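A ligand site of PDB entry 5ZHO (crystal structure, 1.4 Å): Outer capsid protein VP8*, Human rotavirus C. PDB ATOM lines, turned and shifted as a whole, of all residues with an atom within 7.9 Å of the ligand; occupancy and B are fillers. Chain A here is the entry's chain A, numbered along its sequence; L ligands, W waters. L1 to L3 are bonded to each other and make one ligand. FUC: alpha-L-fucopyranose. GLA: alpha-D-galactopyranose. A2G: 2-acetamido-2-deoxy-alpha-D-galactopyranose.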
ATOM      1  N   HIS A  38      21.525   8.521 -15.043  1.00  0.00           N
ATOM      2  CA  HIS A  38      20.344   8.066 -14.336  1.00  0.00           C
ATOM      3  C   HIS A  38      20.372   6.546 -14.337  1.00  0.00           C
ATOM      4  O   HIS A  38      20.286   5.921 -15.398  1.00  0.00           O
ATOM      5  CB  HIS A  38      19.065   8.568 -15.008  1.00  0.00           C
ATOM      6  CG  HIS A  38      17.816   8.054 -14.359  1.00  0.00           C
ATOM      7  ND1 HIS A  38      17.470   8.355 -13.065  1.00  0.00           N
ATOM      8  CD2 HIS A  38      16.839   7.245 -14.832  1.00  0.00           C
ATOM      9  CE1 HIS A  38      16.334   7.761 -12.767  1.00  0.00           C
ATOM     10  NE2 HIS A  38      15.929   7.071 -13.810  1.00  0.00           N
ATOM     11  N   PRO A  40      21.246   2.861 -11.387  1.00  0.00           N
ATOM     12  CA  PRO A  40      21.907   2.394 -10.167  1.00  0.00           C
ATOM     13  C   PRO A  40      23.410   2.588 -10.249  1.00  0.00           C
ATOM     14  O   PRO A  40      23.970   2.953 -11.290  1.00  0.00           O
ATOM     15  CB  PRO A  40      21.529   0.907 -10.117  1.00  0.00           C
ATOM     16  CG  PRO A  40      21.321   0.522 -11.529  1.00  0.00           C
ATOM     17  CD  PRO A  40      20.728   1.746 -12.199  1.00  0.00           C
ATOM     18  N   ASN A  44      22.641  -2.777 -14.106  1.00  0.00           N
ATOM     19  CA  ASN A  44      21.588  -3.749 -13.833  1.00  0.00           C
ATOM     20  C   ASN A  44      20.686  -3.788 -15.057  1.00  0.00           C
ATOM     21  O   ASN A  44      19.907  -2.877 -15.301  1.00  0.00           O
ATOM     22  CB  ASN A  44      20.785  -3.332 -12.600  1.00  0.00           C
ATOM     23  CG  ASN A  44      19.716  -4.344 -12.239  1.00  0.00           C
ATOM     24  OD1 ASN A  44      19.396  -5.234 -13.017  1.00  0.00           O
ATOM     25  ND2 ASN A  44      19.152  -4.200 -11.048  1.00  0.00           N
ATOM     26  N   SER A  45      20.793  -4.884 -15.829  1.00  0.00           N
ATOM     27  CA  SER A  45      20.054  -5.006 -17.079  1.00  0.00           C
ATOM     28  C   SER A  45      18.548  -5.031 -16.878  1.00  0.00           C
ATOM     29  O   SER A  45      17.801  -4.835 -17.839  1.00  0.00           O
ATOM     30  CB  SER A  45      20.498  -6.270 -17.805  1.00  0.00           C
ATOM     31  OG  SER A  45      20.135  -7.425 -17.076  1.00  0.00           O
ATOM     32  N   ASN A  46      18.069  -5.241 -15.656  1.00  0.00           N
ATOM     33  CA  ASN A  46      16.637  -5.211 -15.407  1.00  0.00           C
ATOM     34  C   ASN A  46      16.061  -3.805 -15.390  1.00  0.00           C
ATOM     35  O   ASN A  46      14.840  -3.657 -15.489  1.00  0.00           O
ATOM     36  CB  ASN A  46      16.327  -5.868 -14.068  1.00  0.00           C
ATOM     37  CG  ASN A  46      16.614  -7.351 -14.072  1.00  0.00           C
ATOM     38  OD1 ASN A  46      16.336  -8.041 -15.046  1.00  0.00           O
ATOM     39  ND2 ASN A  46      17.175  -7.840 -12.973  1.00  0.00           N
ATOM     40  N   LEU A  47      16.905  -2.791 -15.273  1.00  0.00           N
ATOM     41  CA  LEU A  47      16.453  -1.421 -15.092  1.00  0.00           C
ATOM     42  C   LEU A  47      16.779  -0.588 -16.321  1.00  0.00           C
ATOM     43  O   LEU A  47      17.820  -0.777 -16.952  1.00  0.00           O
ATOM     44  CB  LEU A  47      17.137  -0.794 -13.878  1.00  0.00           C
ATOM     45  CG  LEU A  47      16.996  -1.588 -12.565  1.00  0.00           C
ATOM     46  CD1 LEU A  47      17.599  -0.836 -11.385  1.00  0.00           C
ATOM     47  CD2 LEU A  47      15.548  -1.933 -12.276  1.00  0.00           C
ATOM     48  N   ALA A  48      15.907   0.370 -16.630  1.00  0.00           N
ATOM     49  CA  ALA A  48      16.221   1.402 -17.595  1.00  0.00           C
ATOM     50  C   ALA A  48      17.269   2.349 -17.031  1.00  0.00           C
ATOM     51  O   ALA A  48      17.331   2.590 -15.823  1.00  0.00           O
ATOM     52  CB  ALA A  48      14.954   2.199 -17.928  1.00  0.00           C
ATOM     53  N   ALA A  49      18.089   2.901 -17.926  1.00  0.00           N
ATOM     54  CA  ALA A  49      19.164   3.799 -17.503  1.00  0.00           C
ATOM     55  C   ALA A  49      19.632   4.632 -18.689  1.00  0.00           C
ATOM     56  O   ALA A  49      19.371   4.310 -19.847  1.00  0.00           O
ATOM     57  CB  ALA A  49      20.343   3.009 -16.918  1.00  0.00           C
ATOM     58  N   ASN A  88      19.475   2.494 -22.217  1.00  0.00           N
ATOM     59  CA  ASN A  88      18.730   1.248 -22.325  1.00  0.00           C
ATOM     60  C   ASN A  88      17.374   1.435 -21.683  1.00  0.00           C
ATOM     61  O   ASN A  88      17.238   2.148 -20.685  1.00  0.00           O
ATOM     62  CB  ASN A  88      19.468   0.051 -21.703  1.00  0.00           C
ATOM     63  CG  ASN A  88      19.328  -0.008 -20.193  1.00  0.00           C
ATOM     64  OD1 ASN A  88      20.074   0.625 -19.454  1.00  0.00           O
ATOM     65  ND2 ASN A  88      18.359  -0.800 -19.728  1.00  0.00           N
ATOM     66  N   GLU A  89      16.364   0.796 -22.266  1.00  0.00           N
ATOM     67  CA  GLU A  89      15.001   0.842 -21.752  1.00  0.00           C
ATOM     68  C   GLU A  89      14.215  -0.268 -22.433  1.00  0.00           C
ATOM     69  O   GLU A  89      14.465  -0.563 -23.606  1.00  0.00           O
ATOM     70  CB  GLU A  89      14.363   2.199 -22.055  1.00  0.00           C
ATOM     71  CG  GLU A  89      12.995   2.394 -21.470  1.00  0.00           C
ATOM     72  CD  GLU A  89      11.879   1.906 -22.359  1.00  0.00           C
ATOM     73  OE1 GLU A  89      12.063   1.907 -23.598  1.00  0.00           O
ATOM     74  OE2 GLU A  89      10.809   1.532 -21.825  1.00  0.00           O
ATOM     75  N   GLY A  90      13.277  -0.856 -21.695  1.00  0.00           N
ATOM     76  CA  GLY A  90      12.446  -1.900 -22.270  1.00  0.00           C
ATOM     77  C   GLY A  90      13.308  -3.032 -22.810  1.00  0.00           C
ATOM     78  O   GLY A  90      14.227  -3.514 -22.148  1.00  0.00           O
ATOM     79  N   SER A  91      13.034  -3.472 -24.038  1.00  0.00           N
ATOM     80  CA  SER A  91      13.786  -4.552 -24.628  1.00  0.00           C
ATOM     81  C   SER A  91      15.014  -4.084 -25.408  1.00  0.00           C
ATOM     82  O   SER A  91      15.653  -4.890 -26.089  1.00  0.00           O
ATOM     83  CB  SER A  91      12.888  -5.417 -25.521  1.00  0.00           C
ATOM     84  OG  SER A  91      12.259  -4.632 -26.507  1.00  0.00           O
ATOM     85  N   THR A  92      15.367  -2.791 -25.324  1.00  0.00           N
ATOM     86  CA  THR A  92      16.589  -2.299 -25.946  1.00  0.00           C
ATOM     87  C   THR A  92      17.764  -2.501 -24.998  1.00  0.00           C
ATOM     88  O   THR A  92      17.819  -1.879 -23.940  1.00  0.00           O
ATOM     89  CB  THR A  92      16.421  -0.821 -26.294  1.00  0.00           C
ATOM     90  OG1 THR A  92      15.382  -0.678 -27.260  1.00  0.00           O
ATOM     91  CG2 THR A  92      17.711  -0.252 -26.864  1.00  0.00           C
ATOM     92  N   SER A 116       6.495   9.254 -13.185  1.00  0.00           N
ATOM     93  CA  SER A 116       7.506   8.206 -13.251  1.00  0.00           C
ATOM     94  C   SER A 116       8.027   7.969 -14.659  1.00  0.00           C
ATOM     95  O   SER A 116       8.604   6.912 -14.927  1.00  0.00           O
ATOM     96  CB  SER A 116       6.943   6.892 -12.683  1.00  0.00           C
ATOM     97  OG  SER A 116       5.854   6.453 -13.455  1.00  0.00           O
ATOM     98  N   ARG A 117       7.878   8.940 -15.564  1.00  0.00           N
ATOM     99  CA  ARG A 117       8.284   8.752 -16.954  1.00  0.00           C
ATOM    100  C   ARG A 117       8.681  10.089 -17.536  1.00  0.00           C
ATOM    101  O   ARG A 117       7.962  11.082 -17.384  1.00  0.00           O
ATOM    102  CB  ARG A 117       7.136   8.136 -17.758  1.00  0.00           C
ATOM    103  CG  ARG A 117       7.523   7.629 -19.130  1.00  0.00           C
ATOM    104  CD  ARG A 117       6.382   6.841 -19.751  1.00  0.00           C
ATOM    105  NE  ARG A 117       6.803   6.078 -20.932  1.00  0.00           N
ATOM    106  CZ  ARG A 117       7.301   4.846 -20.893  1.00  0.00           C
ATOM    107  NH1 ARG A 117       7.654   4.239 -22.013  1.00  0.00           N
ATOM    108  NH2 ARG A 117       7.456   4.211 -19.733  1.00  0.00           N
ATOM    109  N   GLU A 141      11.322   7.923 -24.535  1.00  0.00           N
ATOM    110  CA  GLU A 141      10.656   7.895 -23.234  1.00  0.00           C
ATOM    111  C   GLU A 141      11.347   6.884 -22.323  1.00  0.00           C
ATOM    112  O   GLU A 141      11.564   5.728 -22.705  1.00  0.00           O
ATOM    113  CB  GLU A 141       9.192   7.503 -23.388  1.00  0.00           C
ATOM    114  CG  GLU A 141       8.375   8.363 -24.315  1.00  0.00           C
ATOM    115  CD  GLU A 141       6.880   8.107 -24.174  1.00  0.00           C
ATOM    116  OE1 GLU A 141       6.474   7.359 -23.252  1.00  0.00           O
ATOM    117  OE2 GLU A 141       6.107   8.657 -24.990  1.00  0.00           O
ATOM    118  N   PHE A 142      11.648   7.317 -21.110  1.00  0.00           N
ATOM    119  CA  PHE A 142      12.260   6.469 -20.093  1.00  0.00           C
ATOM    120  C   PHE A 142      11.361   6.423 -18.872  1.00  0.00           C
ATOM    121  O   PHE A 142      10.972   7.473 -18.346  1.00  0.00           O
ATOM    122  CB  PHE A 142      13.616   7.031 -19.684  1.00  0.00           C
ATOM    123  CG  PHE A 142      14.649   6.915 -20.757  1.00  0.00           C
ATOM    124  CD1 PHE A 142      14.791   7.910 -21.698  1.00  0.00           C
ATOM    125  CD2 PHE A 142      15.479   5.805 -20.830  1.00  0.00           C
ATOM    126  CE1 PHE A 142      15.730   7.815 -22.690  1.00  0.00           C
ATOM    127  CE2 PHE A 142      16.420   5.705 -21.809  1.00  0.00           C
ATOM    128  CZ  PHE A 142      16.543   6.710 -22.750  1.00  0.00           C
ATOM    129  N   PRO A 143      11.042   5.244 -18.355  1.00  0.00           N
ATOM    130  CA  PRO A 143      10.531   5.159 -16.989  1.00  0.00           C
ATOM    131  C   PRO A 143      11.668   5.427 -16.033  1.00  0.00           C
ATOM    132  O   PRO A 143      12.837   5.233 -16.347  1.00  0.00           O
ATOM    133  CB  PRO A 143      10.063   3.704 -16.886  1.00  0.00           C
ATOM    134  CG  PRO A 143      11.059   2.973 -17.742  1.00  0.00           C
ATOM    135  CD  PRO A 143      11.424   3.906 -18.867  1.00  0.00           C
ATOM    136  N   ARG A 144      11.310   5.891 -14.840  1.00  0.00           N
ATOM    137  CA  ARG A 144      12.322   6.007 -13.798  1.00  0.00           C
ATOM    138  C   ARG A 144      12.990   4.654 -13.593  1.00  0.00           C
ATOM    139  O   ARG A 144      12.347   3.604 -13.577  1.00  0.00           O
ATOM    140  CB  ARG A 144      11.679   6.485 -12.508  1.00  0.00           C
ATOM    141  CG  ARG A 144      12.673   7.026 -11.488  1.00  0.00           C
ATOM    142  CD  ARG A 144      11.981   7.459 -10.223  1.00  0.00           C
ATOM    143  NE  ARG A 144      12.901   8.119  -9.303  1.00  0.00           N
ATOM    144  CZ  ARG A 144      12.556   8.578  -8.099  1.00  0.00           C
ATOM    145  NH1 ARG A 144      11.317   8.420  -7.662  1.00  0.00           N
ATOM    146  NH2 ARG A 144      13.458   9.171  -7.336  1.00  0.00           N
ATOM    147  N   SER A 145      14.318   4.676 -13.482  1.00  0.00           N
ATOM    148  CA  SER A 145      15.096   3.436 -13.374  1.00  0.00           C
ATOM    149  C   SER A 145      14.529   2.544 -12.295  1.00  0.00           C
ATOM    150  O   SER A 145      14.321   1.336 -12.496  1.00  0.00           O
ATOM    151  CB  SER A 145      16.557   3.798 -13.084  1.00  0.00           C
ATOM    152  OG  SER A 145      17.376   2.634 -13.053  1.00  0.00           O
ATOM    153  N   ASN A 146      14.254   3.107 -11.131  1.00  0.00           N
ATOM    154  CA  ASN A 146      13.470   2.464 -10.095  1.00  0.00           C
ATOM    155  C   ASN A 146      13.151   3.517  -9.052  1.00  0.00           C
ATOM    156  O   ASN A 146      13.734   4.617  -9.076  1.00  0.00           O
ATOM    157  CB  ASN A 146      14.235   1.288  -9.499  1.00  0.00           C
ATOM    158  CG  ASN A 146      13.492  -0.030  -9.622  1.00  0.00           C
ATOM    159  OD1 ASN A 146      12.459  -0.141 -10.292  1.00  0.00           O
ATOM    160  ND2 ASN A 146      14.024  -1.055  -8.967  1.00  0.00           N
ATOM    161  N   PRO A 147      12.246   3.239  -8.121  1.00  0.00           N
ATOM    162  CA  PRO A 147      11.966   4.213  -7.064  1.00  0.00           C
ATOM    163  C   PRO A 147      13.235   4.631  -6.350  1.00  0.00           C
ATOM    164  O   PRO A 147      14.128   3.827  -6.089  1.00  0.00           O
ATOM    165  CB  PRO A 147      11.006   3.455  -6.136  1.00  0.00           C
ATOM    166  CG  PRO A 147      10.316   2.492  -7.038  1.00  0.00           C
ATOM    167  CD  PRO A 147      11.373   2.061  -8.037  1.00  0.00           C
ATOM    168  N   ILE A 149      15.721   6.472  -7.391  1.00  0.00           N
ATOM    169  CA  ILE A 149      16.885   6.755  -8.221  1.00  0.00           C
ATOM    170  C   ILE A 149      16.719   8.132  -8.860  1.00  0.00           C
ATOM    171  O   ILE A 149      15.728   8.404  -9.548  1.00  0.00           O
ATOM    172  CB  ILE A 149      17.105   5.642  -9.270  1.00  0.00           C
ATOM    173  CG1 ILE A 149      17.358   4.312  -8.526  1.00  0.00           C
ATOM    174  CG2 ILE A 149      18.276   5.969 -10.176  1.00  0.00           C
ATOM    175  CD1 ILE A 149      17.608   3.125  -9.417  1.00  0.00           C
HETATM  176  C1  FUC L   1      12.415  -4.324 -12.781  1.00  0.00           C
HETATM  177  C2  FUC L   1      12.440  -3.545 -11.482  1.00  0.00           C
HETATM  178  C3  FUC L   1      12.039  -4.424 -10.304  1.00  0.00           C
HETATM  179  C4  FUC L   1      12.936  -5.648 -10.266  1.00  0.00           C
HETATM  180  C5  FUC L   1      12.854  -6.380 -11.605  1.00  0.00           C
HETATM  181  C6  FUC L   1      13.782  -7.594 -11.624  1.00  0.00           C
HETATM  182  O2  FUC L   1      11.534  -2.439 -11.567  1.00  0.00           O
HETATM  183  O3  FUC L   1      12.175  -3.672  -9.098  1.00  0.00           O
HETATM  184  O4  FUC L   1      14.288  -5.243 -10.023  1.00  0.00           O
HETATM  185  O5  FUC L   1      13.216  -5.512 -12.679  1.00  0.00           O
HETATM  186  C1  GLA L   2      10.006  -6.325 -14.378  1.00  0.00           C
HETATM  187  C2  GLA L   2      10.901  -5.096 -14.421  1.00  0.00           C
HETATM  188  C3  GLA L   2      10.313  -4.009 -15.312  1.00  0.00           C
HETATM  189  C4  GLA L   2       9.871  -4.568 -16.660  1.00  0.00           C
HETATM  190  C5  GLA L   2       9.084  -5.882 -16.517  1.00  0.00           C
HETATM  191  C6  GLA L   2       8.869  -6.558 -17.870  1.00  0.00           C
HETATM  192  O1  GLA L   2       8.750  -5.958 -13.804  1.00  0.00           O
HETATM  193  O2  GLA L   2      11.039  -4.611 -13.079  1.00  0.00           O
HETATM  194  O3  GLA L   2      11.342  -3.019 -15.465  1.00  0.00           O
HETATM  195  O4  GLA L   2      11.008  -4.799 -17.497  1.00  0.00           O
HETATM  196  O5  GLA L   2       9.812  -6.801 -15.698  1.00  0.00           O
HETATM  197  O6  GLA L   2       7.877  -5.842 -18.614  1.00  0.00           O
HETATM  198  O5  A2G L   3       9.856  -1.124 -15.401  1.00  0.00           O
HETATM  199  C1  A2G L   3      10.909  -1.800 -16.104  1.00  0.00           C
HETATM  200  C2  A2G L   3      12.130  -0.891 -16.202  1.00  0.00           C
HETATM  201  N2  A2G L   3      13.224  -1.596 -16.848  1.00  0.00           N
HETATM  202  C3  A2G L   3      12.542  -0.463 -14.802  1.00  0.00           C
HETATM  203  O3  A2G L   3      13.676   0.425 -14.869  1.00  0.00           O
HETATM  204  C4  A2G L   3      11.399   0.243 -14.101  1.00  0.00           C
HETATM  205  O4  A2G L   3      11.054   1.449 -14.801  1.00  0.00           O
HETATM  206  C5  A2G L   3      10.192  -0.686 -14.076  1.00  0.00           C
HETATM  207  C6  A2G L   3       8.977   0.004 -13.461  1.00  0.00           C
HETATM  208  O6  A2G L   3       7.968  -0.989 -13.212  1.00  0.00           O
HETATM  209  C7  A2G L   3      13.507  -1.465 -18.144  1.00  0.00           C
HETATM  210  O7  A2G L   3      12.915  -0.675 -18.862  1.00  0.00           O
HETATM  211  C8  A2G L   3      14.619  -2.341 -18.654  1.00  0.00           C
HETATM  212  O   HOH W   1       7.109  -3.131 -18.663  1.00  0.00           O
HETATM  213  O   HOH W   2      16.724  -5.976 -10.472  1.00  0.00           O
HETATM  214  O   HOH W   3      10.713  -4.418 -20.276  1.00  0.00           O
HETATM  215  O   HOH W   4       9.707   3.465 -12.559  1.00  0.00           O
HETATM  216  O   HOH W   5      10.400  -0.178 -19.609  1.00  0.00           O
HETATM  217  O   HOH W   6       8.883  -3.089 -11.576  1.00  0.00           O
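A nitrogen (N2) of A2G L3 sits at hydrogen-bond distance from the backbone carbonyl oxygen (O) of Asn 46 (3.0 Å). The backbone NH (N) of Ala 48 sits at hydrogen-bond distance from an oxygen (O3) of A2G L3. O3 of A2G L3 sits at hydrogen-bond distance from O of Ser 145. An oxygen (O4) of A2G L3 sits at hydrogen-bond distance from the backbone carbonyl oxygen (O) of Arg 144 (2.8 Å). OD1 of Asn 146 sits at hydrogen-bond distance from O2 of FUC L1 (2.8 Å). The backbone NH (N) of Gly 90 is in hydrogen-bond range of an oxygen (O7) of A2G L3 (2.9 Å).
The backbone NH (N) of Arg 144 lies within hydrogen-bond range of the backbone carbonyl oxygen (O) of Ser 116, 2.9 Å away. O of Ala 48 lies within hydrogen-bond range of OG of Ser 145 (2.8 Å). A ring nitrogen (NE2) of His 38 lies within hydrogen-bond range of the backbone NH (N) of Ser 145, 2.9 Å away. The backbone NH (N) of Asn 46 is in hydrogen-bond range of the side-chain amide oxygen (OD1) of Asn 44, 3.0 Å away. ND2 of Asn 88 is in hydrogen-bond range of O of Leu 47, 2.8 Å away. The guanidinium group (NE) of Arg 144 lies within hydrogen-bond range of the backbone carbonyl oxygen (O) of Ile 149 (2.9 Å).
Residues that only touch the ligand: Leu 47 (3.3 Å), Glu 89 (3.8 Å) and Pro 143 (3.2 Å). Hydrophobic or aromatic side chains that line the ligand: Leu 47, Ala 48 and Pro 143. Within 4 Å of the ligand: Asn 46, Leu 47, Ala 48, Glu 89, Gly 90, Pro 143, Arg 144, Ser 145 and Asn 146. The nearest printed residue that does not touch the ligand is Ser 45 (4.1 Å).
Water W2 lies within hydrogen-bond range of an oxygen (O4) of FUC L1 (2.6 Å), the side-chain amide nitrogen (ND2) of Asn 44 (3.1 Å) and the side-chain amide nitrogen (ND2) of Asn 46 (3.2 Å). Water W5 lies within hydrogen-bond range of an oxygen (O7) of A2G L3 (2.7 Å) and the side-chain carboxylate of Glu 89 (2.8 Å). Water W4 lies within hydrogen-bond range of the backbone carbonyl oxygen (O) of Arg 144 and an oxygen (O4) of A2G L3.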
